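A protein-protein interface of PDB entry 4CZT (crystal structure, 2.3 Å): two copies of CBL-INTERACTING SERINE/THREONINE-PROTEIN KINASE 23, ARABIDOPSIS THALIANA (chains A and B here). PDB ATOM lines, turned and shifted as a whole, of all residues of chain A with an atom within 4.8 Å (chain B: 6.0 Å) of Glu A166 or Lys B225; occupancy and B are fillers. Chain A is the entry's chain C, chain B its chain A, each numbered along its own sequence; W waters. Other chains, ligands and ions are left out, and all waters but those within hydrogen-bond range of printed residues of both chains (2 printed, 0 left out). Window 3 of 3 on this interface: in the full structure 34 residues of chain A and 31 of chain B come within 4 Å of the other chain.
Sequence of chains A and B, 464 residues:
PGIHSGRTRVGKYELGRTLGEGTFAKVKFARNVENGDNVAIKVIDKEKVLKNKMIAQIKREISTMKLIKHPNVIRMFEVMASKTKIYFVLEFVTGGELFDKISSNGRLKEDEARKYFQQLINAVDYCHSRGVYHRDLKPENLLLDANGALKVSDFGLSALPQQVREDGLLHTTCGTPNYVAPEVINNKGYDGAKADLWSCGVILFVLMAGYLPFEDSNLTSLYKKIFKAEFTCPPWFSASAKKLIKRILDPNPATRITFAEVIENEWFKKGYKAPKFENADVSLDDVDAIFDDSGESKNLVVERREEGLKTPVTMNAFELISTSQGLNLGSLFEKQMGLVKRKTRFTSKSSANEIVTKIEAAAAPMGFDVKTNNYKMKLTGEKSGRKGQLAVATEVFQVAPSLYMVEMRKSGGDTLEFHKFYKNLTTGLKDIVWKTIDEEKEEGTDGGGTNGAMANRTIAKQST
The backbone carbonyl oxygen of Glu B215 is in hydrogen-bond range of the side-chain amide nitrogen of Gln A162. The side-chain amino group of Lys B225 lies within salt-bridge range of the side-chain carboxylate of Glu A166 (3.2 Å). OE2 of Glu A166 sits close to O of Glu B215, at 3.5 Å.
The side-chain amino group (NZ) of Lys B225 lies within hydrogen-bond range of the backbone carbonyl oxygen (O) of Glu B215 (2.6 Å). NZ of Lys B225 is in salt-bridge range of OD2 of Asp B216. The backbone carbonyl oxygen of Lys B225 is in hydrogen-bond range of the backbone NH of Glu B230 (2.9 Å). OE1 of Gln A162 is in hydrogen-bond range of NH2 of Arg A165, at 2.7 Å. NE2 of Gln A162 lies within hydrogen-bond range of OE2 of Glu A166, at 2.6 Å.
Among the printed residues, merely in contact across the chains: Gln A162 with Asp B216.
Printed residues of chain B within 4 Å of Gln A162: Glu B215 and Asp B216. Glu A166 touches two residues of chain B. Of the printed residues of chain A, Glu B215 touches Gln A162 and Glu A166. Of the printed residues of chain A, Asp B216 touches Gln A162 (3.6 Å). Printed residues of chain A within 4 Å of Lys B225: Glu A166. The nearest residue of chain B that does not touch Glu A166 is Asp B216 (5.2 Å).
Of the 16 printed residues of chain B, 3 touch a printed residue of chain A. Of the 10 printed residues of chain A, 2 touch a printed residue of chain B. Printed residues of chain A that touch a printed residue of chain B: Gln A162 and Glu A166. Among the printed residues, 4 pairs touch across the chains. Among the printed residues, Asp or Glu carboxylates within 4 Å of a Lys or Arg side-chain nitrogen of the other chain: Glu A166 with Lys B225 (3.2 Å).
No position is printed for both chains. Of the 4 pairs that touch across the chains among the printed residues, none has its exchanged pair printed and touching as well.
Water W1 lies within hydrogen-bond range of the side-chain carboxylate of Glu B215, the backbone NH of Asp A167 and the backbone NH of Gly A168. Water W2 lies within hydrogen-bond range of the backbone NH (N) of Glu B215 (2.9 Å), the backbone carbonyl oxygen (O) of Pro B213 (3.4 Å), the side-chain amino group (NZ) of Lys B225 (3.4 Å) and the side-chain carboxylate (OE2) of Glu A166 (3.5 Å).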
ATOM      1  N   GLY A  22      12.907 -22.669 -21.805  1.00  0.00           N
ATOM      2  CA  GLY A  22      14.152 -22.306 -21.157  1.00  0.00           C
ATOM      3  C   GLY A  22      14.799 -23.511 -20.502  1.00  0.00           C
ATOM      4  O   GLY A  22      14.319 -24.639 -20.619  1.00  0.00           O
ATOM      5  N   THR A  23      15.895 -23.268 -19.800  1.00  0.00           N
ATOM      6  CA  THR A  23      16.689 -24.341 -19.227  1.00  0.00           C
ATOM      7  C   THR A  23      15.997 -25.053 -18.057  1.00  0.00           C
ATOM      8  O   THR A  23      16.052 -26.278 -17.974  1.00  0.00           O
ATOM      9  CB  THR A  23      18.061 -23.805 -18.777  1.00  0.00           C
ATOM     10  OG1 THR A  23      18.771 -23.305 -19.919  1.00  0.00           O
ATOM     11  CG2 THR A  23      18.879 -24.893 -18.146  1.00  0.00           C
ATOM     12  N   ALA A  25      12.680 -24.120 -17.105  1.00  0.00           N
ATOM     13  CA  ALA A  25      11.270 -23.801 -17.194  1.00  0.00           C
ATOM     14  C   ALA A  25      10.895 -23.685 -18.635  1.00  0.00           C
ATOM     15  O   ALA A  25      11.741 -23.415 -19.496  1.00  0.00           O
ATOM     16  CB  ALA A  25      10.952 -22.507 -16.457  1.00  0.00           C
ATOM     17  N   GLN A 162      15.354 -16.394 -10.157  1.00  0.00           N
ATOM     18  CA  GLN A 162      15.588 -15.820 -11.474  1.00  0.00           C
ATOM     19  C   GLN A 162      15.755 -16.912 -12.539  1.00  0.00           C
ATOM     20  O   GLN A 162      15.330 -16.752 -13.680  1.00  0.00           O
ATOM     21  CB  GLN A 162      16.814 -14.905 -11.421  1.00  0.00           C
ATOM     22  CG  GLN A 162      17.377 -14.504 -12.768  1.00  0.00           C
ATOM     23  CD  GLN A 162      16.384 -13.728 -13.616  1.00  0.00           C
ATOM     24  OE1 GLN A 162      15.561 -12.961 -13.101  1.00  0.00           O
ATOM     25  NE2 GLN A 162      16.456 -13.928 -14.926  1.00  0.00           N
ATOM     26  N   GLN A 163      16.335 -18.036 -12.146  1.00  0.00           N
ATOM     27  CA  GLN A 163      16.584 -19.132 -13.072  1.00  0.00           C
ATOM     28  C   GLN A 163      15.329 -19.876 -13.552  1.00  0.00           C
ATOM     29  O   GLN A 163      15.397 -20.582 -14.552  1.00  0.00           O
ATOM     30  CB  GLN A 163      17.555 -20.133 -12.441  1.00  0.00           C
ATOM     31  CG  GLN A 163      19.016 -19.812 -12.696  1.00  0.00           C
ATOM     32  CD  GLN A 163      19.952 -20.818 -12.062  1.00  0.00           C
ATOM     33  OE1 GLN A 163      19.595 -21.501 -11.098  1.00  0.00           O
ATOM     34  NE2 GLN A 163      21.156 -20.925 -12.608  1.00  0.00           N
ATOM     35  N   VAL A 164      14.199 -19.741 -12.862  1.00  0.00           N
ATOM     36  CA  VAL A 164      12.968 -20.324 -13.389  1.00  0.00           C
ATOM     37  C   VAL A 164      12.098 -19.222 -13.965  1.00  0.00           C
ATOM     38  O   VAL A 164      11.078 -19.484 -14.599  1.00  0.00           O
ATOM     39  CB  VAL A 164      12.173 -21.120 -12.334  1.00  0.00           C
ATOM     40  CG1 VAL A 164      12.971 -22.337 -11.889  1.00  0.00           C
ATOM     41  CG2 VAL A 164      11.807 -20.244 -11.139  1.00  0.00           C
ATOM     42  N   ARG A 165      12.513 -17.984 -13.755  1.00  0.00           N
ATOM     43  CA  ARG A 165      11.862 -16.857 -14.401  1.00  0.00           C
ATOM     44  C   ARG A 165      12.324 -16.756 -15.859  1.00  0.00           C
ATOM     45  O   ARG A 165      11.673 -16.108 -16.681  1.00  0.00           O
ATOM     46  CB  ARG A 165      12.154 -15.567 -13.643  1.00  0.00           C
ATOM     47  CG  ARG A 165      10.958 -15.008 -12.901  1.00  0.00           C
ATOM     48  CD  ARG A 165      11.354 -14.419 -11.554  1.00  0.00           C
ATOM     49  NE  ARG A 165      12.555 -13.580 -11.626  1.00  0.00           N
ATOM     50  CZ  ARG A 165      13.236 -13.147 -10.564  1.00  0.00           C
ATOM     51  NH1 ARG A 165      12.846 -13.473  -9.332  1.00  0.00           N
ATOM     52  NH2 ARG A 165      14.317 -12.394 -10.732  1.00  0.00           N
ATOM     53  N   GLU A 166      13.446 -17.408 -16.171  1.00  0.00           N
ATOM     54  CA  GLU A 166      13.935 -17.525 -17.546  1.00  0.00           C
ATOM     55  C   GLU A 166      13.275 -18.720 -18.216  1.00  0.00           C
ATOM     56  O   GLU A 166      13.850 -19.797 -18.318  1.00  0.00           O
ATOM     57  CB  GLU A 166      15.457 -17.658 -17.565  1.00  0.00           C
ATOM     58  CG  GLU A 166      16.172 -16.353 -17.194  1.00  0.00           C
ATOM     59  CD  GLU A 166      17.584 -16.566 -16.658  1.00  0.00           C
ATOM     60  OE1 GLU A 166      18.133 -17.681 -16.821  1.00  0.00           O
ATOM     61  OE2 GLU A 166      18.144 -15.615 -16.064  1.00  0.00           O
ATOM     62  N   ASP A 167      12.048 -18.508 -18.671  1.00  0.00           N
ATOM     63  CA  ASP A 167      11.163 -19.576 -19.099  1.00  0.00           C
ATOM     64  C   ASP A 167      11.101 -19.735 -20.625  1.00  0.00           C
ATOM     65  O   ASP A 167      10.159 -20.340 -21.147  1.00  0.00           O
ATOM     66  CB  ASP A 167       9.766 -19.302 -18.561  1.00  0.00           C
ATOM     67  CG  ASP A 167       9.339 -17.848 -18.771  1.00  0.00           C
ATOM     68  OD1 ASP A 167      10.049 -17.109 -19.505  1.00  0.00           O
ATOM     69  OD2 ASP A 167       8.288 -17.448 -18.220  1.00  0.00           O
ATOM     70  N   GLY A 168      12.085 -19.181 -21.331  1.00  0.00           N
ATOM     71  CA  GLY A 168      12.143 -19.280 -22.780  1.00  0.00           C
ATOM     72  C   GLY A 168      11.346 -18.226 -23.535  1.00  0.00           C
ATOM     73  O   GLY A 168      11.428 -18.153 -24.752  1.00  0.00           O
ATOM     74  N   PRO B 213      19.815 -13.604 -24.365  1.00  0.00           N
ATOM     75  CA  PRO B 213      20.961 -14.316 -23.785  1.00  0.00           C
ATOM     76  C   PRO B 213      21.395 -13.761 -22.413  1.00  0.00           C
ATOM     77  O   PRO B 213      21.909 -14.502 -21.559  1.00  0.00           O
ATOM     78  CB  PRO B 213      22.072 -14.098 -24.828  1.00  0.00           C
ATOM     79  CG  PRO B 213      21.703 -12.805 -25.499  1.00  0.00           C
ATOM     80  CD  PRO B 213      20.190 -12.809 -25.554  1.00  0.00           C
ATOM     81  N   PHE B 214      21.212 -12.461 -22.220  1.00  0.00           N
ATOM     82  CA  PHE B 214      21.483 -11.825 -20.931  1.00  0.00           C
ATOM     83  C   PHE B 214      20.230 -11.144 -20.450  1.00  0.00           C
ATOM     84  O   PHE B 214      19.736 -10.212 -21.093  1.00  0.00           O
ATOM     85  CB  PHE B 214      22.610 -10.800 -21.028  1.00  0.00           C
ATOM     86  CG  PHE B 214      23.739 -11.225 -21.912  1.00  0.00           C
ATOM     87  CD1 PHE B 214      24.623 -12.203 -21.502  1.00  0.00           C
ATOM     88  CD2 PHE B 214      23.913 -10.641 -23.159  1.00  0.00           C
ATOM     89  CE1 PHE B 214      25.665 -12.589 -22.312  1.00  0.00           C
ATOM     90  CE2 PHE B 214      24.950 -11.026 -23.979  1.00  0.00           C
ATOM     91  CZ  PHE B 214      25.828 -12.004 -23.564  1.00  0.00           C
ATOM     92  N   GLU B 215      19.703 -11.611 -19.329  1.00  0.00           N
ATOM     93  CA  GLU B 215      18.515 -10.994 -18.766  1.00  0.00           C
ATOM     94  C   GLU B 215      18.443 -11.235 -17.252  1.00  0.00           C
ATOM     95  O   GLU B 215      18.888 -12.268 -16.755  1.00  0.00           O
ATOM     96  CB  GLU B 215      17.253 -11.512 -19.472  1.00  0.00           C
ATOM     97  CG  GLU B 215      17.042 -13.000 -19.322  1.00  0.00           C
ATOM     98  CD  GLU B 215      15.711 -13.468 -19.899  1.00  0.00           C
ATOM     99  OE1 GLU B 215      14.756 -12.651 -19.964  1.00  0.00           O
ATOM    100  OE2 GLU B 215      15.627 -14.653 -20.290  1.00  0.00           O
ATOM    101  N   ASP B 216      17.901 -10.255 -16.532  1.00  0.00           N
ATOM    102  CA  ASP B 216      17.785 -10.326 -15.077  1.00  0.00           C
ATOM    103  C   ASP B 216      16.972  -9.150 -14.534  1.00  0.00           C
ATOM    104  O   ASP B 216      17.191  -8.002 -14.912  1.00  0.00           O
ATOM    105  CB  ASP B 216      19.172 -10.336 -14.424  1.00  0.00           C
ATOM    106  CG  ASP B 216      19.199 -11.104 -13.103  1.00  0.00           C
ATOM    107  OD1 ASP B 216      18.313 -10.878 -12.246  1.00  0.00           O
ATOM    108  OD2 ASP B 216      20.118 -11.933 -12.924  1.00  0.00           O
ATOM    109  N   THR B 220      22.140  -5.008 -11.243  1.00  0.00           N
ATOM    110  CA  THR B 220      23.503  -5.401 -10.926  1.00  0.00           C
ATOM    111  C   THR B 220      23.837  -6.713 -11.596  1.00  0.00           C
ATOM    112  O   THR B 220      24.872  -6.823 -12.248  1.00  0.00           O
ATOM    113  CB  THR B 220      23.731  -5.548  -9.408  1.00  0.00           C
ATOM    114  OG1 THR B 220      23.445  -4.305  -8.764  1.00  0.00           O
ATOM    115  CG2 THR B 220      25.186  -5.958  -9.109  1.00  0.00           C
ATOM    116  N   SER B 221      22.957  -7.706 -11.443  1.00  0.00           N
ATOM    117  CA  SER B 221      23.185  -9.031 -12.024  1.00  0.00           C
ATOM    118  C   SER B 221      23.146  -8.996 -13.556  1.00  0.00           C
ATOM    119  O   SER B 221      23.930  -9.677 -14.223  1.00  0.00           O
ATOM    120  CB  SER B 221      22.156 -10.036 -11.493  1.00  0.00           C
ATOM    121  OG  SER B 221      22.204 -10.123 -10.078  1.00  0.00           O
ATOM    122  N   LEU B 222      22.235  -8.195 -14.111  1.00  0.00           N
ATOM    123  CA  LEU B 222      22.151  -8.029 -15.559  1.00  0.00           C
ATOM    124  C   LEU B 222      23.494  -7.517 -16.124  1.00  0.00           C
ATOM    125  O   LEU B 222      24.068  -8.136 -17.020  1.00  0.00           O
ATOM    126  CB  LEU B 222      20.994  -7.078 -15.924  1.00  0.00           C
ATOM    127  CG  LEU B 222      20.816  -6.746 -17.413  1.00  0.00           C
ATOM    128  CD1 LEU B 222      20.835  -8.029 -18.252  1.00  0.00           C
ATOM    129  CD2 LEU B 222      19.525  -5.982 -17.664  1.00  0.00           C
ATOM    130  N   TYR B 223      24.009  -6.416 -15.573  1.00  0.00           N
ATOM    131  CA  TYR B 223      25.274  -5.864 -16.047  1.00  0.00           C
ATOM    132  C   TYR B 223      26.426  -6.859 -15.859  1.00  0.00           C
ATOM    133  O   TYR B 223      27.320  -6.921 -16.698  1.00  0.00           O
ATOM    134  CB  TYR B 223      25.608  -4.532 -15.339  1.00  0.00           C
ATOM    135  CG  TYR B 223      24.806  -3.333 -15.817  1.00  0.00           C
ATOM    136  CD1 TYR B 223      25.110  -2.692 -17.013  1.00  0.00           C
ATOM    137  CD2 TYR B 223      23.752  -2.832 -15.061  1.00  0.00           C
ATOM    138  CE1 TYR B 223      24.365  -1.585 -17.455  1.00  0.00           C
ATOM    139  CE2 TYR B 223      23.013  -1.733 -15.485  1.00  0.00           C
ATOM    140  CZ  TYR B 223      23.327  -1.115 -16.679  1.00  0.00           C
ATOM    141  OH  TYR B 223      22.583  -0.036 -17.099  1.00  0.00           O
ATOM    142  N   LYS B 224      26.414  -7.639 -14.777  1.00  0.00           N
ATOM    143  CA  LYS B 224      27.498  -8.603 -14.547  1.00  0.00           C
ATOM    144  C   LYS B 224      27.517  -9.721 -15.592  1.00  0.00           C
ATOM    145  O   LYS B 224      28.583 -10.111 -16.080  1.00  0.00           O
ATOM    146  CB  LYS B 224      27.413  -9.203 -13.140  1.00  0.00           C
ATOM    147  CG  LYS B 224      27.985  -8.257 -12.086  1.00  0.00           C
ATOM    148  CD  LYS B 224      28.022  -8.837 -10.670  1.00  0.00           C
ATOM    149  CE  LYS B 224      28.587  -7.794  -9.681  1.00  0.00           C
ATOM    150  NZ  LYS B 224      28.570  -8.236  -8.251  1.00  0.00           N
ATOM    151  N   LYS B 225      26.337 -10.231 -15.924  1.00  0.00           N
ATOM    152  CA  LYS B 225      26.199 -11.220 -16.977  1.00  0.00           C
ATOM    153  C   LYS B 225      26.803 -10.708 -18.280  1.00  0.00           C
ATOM    154  O   LYS B 225      27.545 -11.425 -18.948  1.00  0.00           O
ATOM    155  CB  LYS B 225      24.727 -11.571 -17.192  1.00  0.00           C
ATOM    156  CG  LYS B 225      24.152 -12.492 -16.162  1.00  0.00           C
ATOM    157  CD  LYS B 225      22.628 -12.509 -16.242  1.00  0.00           C
ATOM    158  CE  LYS B 225      22.040 -13.455 -15.201  1.00  0.00           C
ATOM    159  NZ  LYS B 225      20.580 -13.662 -15.426  1.00  0.00           N
ATOM    160  N   ILE B 226      26.502  -9.453 -18.617  1.00  0.00           N
ATOM    161  CA  ILE B 226      26.931  -8.854 -19.876  1.00  0.00           C
ATOM    162  C   ILE B 226      28.451  -8.695 -19.968  1.00  0.00           C
ATOM    163  O   ILE B 226      29.074  -9.063 -20.979  1.00  0.00           O
ATOM    164  CB  ILE B 226      26.257  -7.479 -20.087  1.00  0.00           C
ATOM    165  CG1 ILE B 226      24.744  -7.670 -20.253  1.00  0.00           C
ATOM    166  CG2 ILE B 226      26.865  -6.777 -21.305  1.00  0.00           C
ATOM    167  CD1 ILE B 226      23.948  -6.391 -20.267  1.00  0.00           C
ATOM    168  N   PHE B 227      29.042  -8.160 -18.906  1.00  0.00           N
ATOM    169  CA  PHE B 227      30.486  -7.972 -18.848  1.00  0.00           C
ATOM    170  C   PHE B 227      31.238  -9.295 -18.945  1.00  0.00           C
ATOM    171  O   PHE B 227      32.327  -9.355 -19.506  1.00  0.00           O
ATOM    172  CB  PHE B 227      30.875  -7.246 -17.556  1.00  0.00           C
ATOM    173  CG  PHE B 227      30.581  -5.777 -17.581  1.00  0.00           C
ATOM    174  CD1 PHE B 227      30.990  -4.997 -18.647  1.00  0.00           C
ATOM    175  CD2 PHE B 227      29.897  -5.174 -16.539  1.00  0.00           C
ATOM    176  CE1 PHE B 227      30.727  -3.640 -18.687  1.00  0.00           C
ATOM    177  CE2 PHE B 227      29.629  -3.812 -16.569  1.00  0.00           C
ATOM    178  CZ  PHE B 227      30.042  -3.045 -17.653  1.00  0.00           C
ATOM    179  N   LYS B 228      30.652 -10.359 -18.408  1.00  0.00           N
ATOM    180  CA  LYS B 228      31.317 -11.651 -18.428  1.00  0.00           C
ATOM    181  C   LYS B 228      30.885 -12.489 -19.612  1.00  0.00           C
ATOM    182  O   LYS B 228      31.410 -13.574 -19.821  1.00  0.00           O
ATOM    183  CB  LYS B 228      31.060 -12.415 -17.127  1.00  0.00           C
ATOM    184  CG  LYS B 228      32.091 -12.107 -16.070  1.00  0.00           C
ATOM    185  CD  LYS B 228      32.252 -13.255 -15.081  1.00  0.00           C
ATOM    186  CE  LYS B 228      33.723 -13.446 -14.672  1.00  0.00           C
ATOM    187  NZ  LYS B 228      34.311 -12.275 -13.959  1.00  0.00           N
ATOM    188  N   ALA B 229      29.940 -11.965 -20.387  1.00  0.00           N
ATOM    189  CA  ALA B 229      29.327 -12.694 -21.495  1.00  0.00           C
ATOM    190  C   ALA B 229      28.885 -14.076 -21.021  1.00  0.00           C
ATOM    191  O   ALA B 229      29.210 -15.104 -21.620  1.00  0.00           O
ATOM    192  CB  ALA B 229      30.279 -12.792 -22.668  1.00  0.00           C
ATOM    193  N   GLU B 230      28.144 -14.078 -19.924  1.00  0.00           N
ATOM    194  CA  GLU B 230      27.680 -15.298 -19.293  1.00  0.00           C
ATOM    195  C   GLU B 230      26.334 -15.679 -19.860  1.00  0.00           C
ATOM    196  O   GLU B 230      25.311 -15.089 -19.525  1.00  0.00           O
ATOM    197  CB  GLU B 230      27.608 -15.100 -17.786  1.00  0.00           C
ATOM    198  CG  GLU B 230      26.860 -16.156 -17.004  1.00  0.00           C
ATOM    199  CD  GLU B 230      26.978 -15.908 -15.504  1.00  0.00           C
ATOM    200  OE1 GLU B 230      28.128 -15.904 -15.008  1.00  0.00           O
ATOM    201  OE2 GLU B 230      25.937 -15.697 -14.829  1.00  0.00           O
ATOM    202  N   PHE B 231      26.337 -16.658 -20.747  1.00  0.00           N
ATOM    203  CA  PHE B 231      25.091 -17.152 -21.291  1.00  0.00           C
ATOM    204  C   PHE B 231      25.203 -18.604 -21.693  1.00  0.00           C
ATOM    205  O   PHE B 231      26.301 -19.156 -21.787  1.00  0.00           O
ATOM    206  CB  PHE B 231      24.671 -16.327 -22.501  1.00  0.00           C
ATOM    207  CG  PHE B 231      25.564 -16.501 -23.690  1.00  0.00           C
ATOM    208  CD1 PHE B 231      26.850 -15.973 -23.694  1.00  0.00           C
ATOM    209  CD2 PHE B 231      25.111 -17.161 -24.820  1.00  0.00           C
ATOM    210  CE1 PHE B 231      27.674 -16.119 -24.789  1.00  0.00           C
ATOM    211  CE2 PHE B 231      25.927 -17.298 -25.929  1.00  0.00           C
ATOM    212  CZ  PHE B 231      27.213 -16.779 -25.913  1.00  0.00           C
HETATM  213  O   HOH W   1      13.034 -15.995 -20.690  1.00  0.00           O
HETATM  214  O   HOH W   2      20.095 -14.466 -18.706  1.00  0.00           O
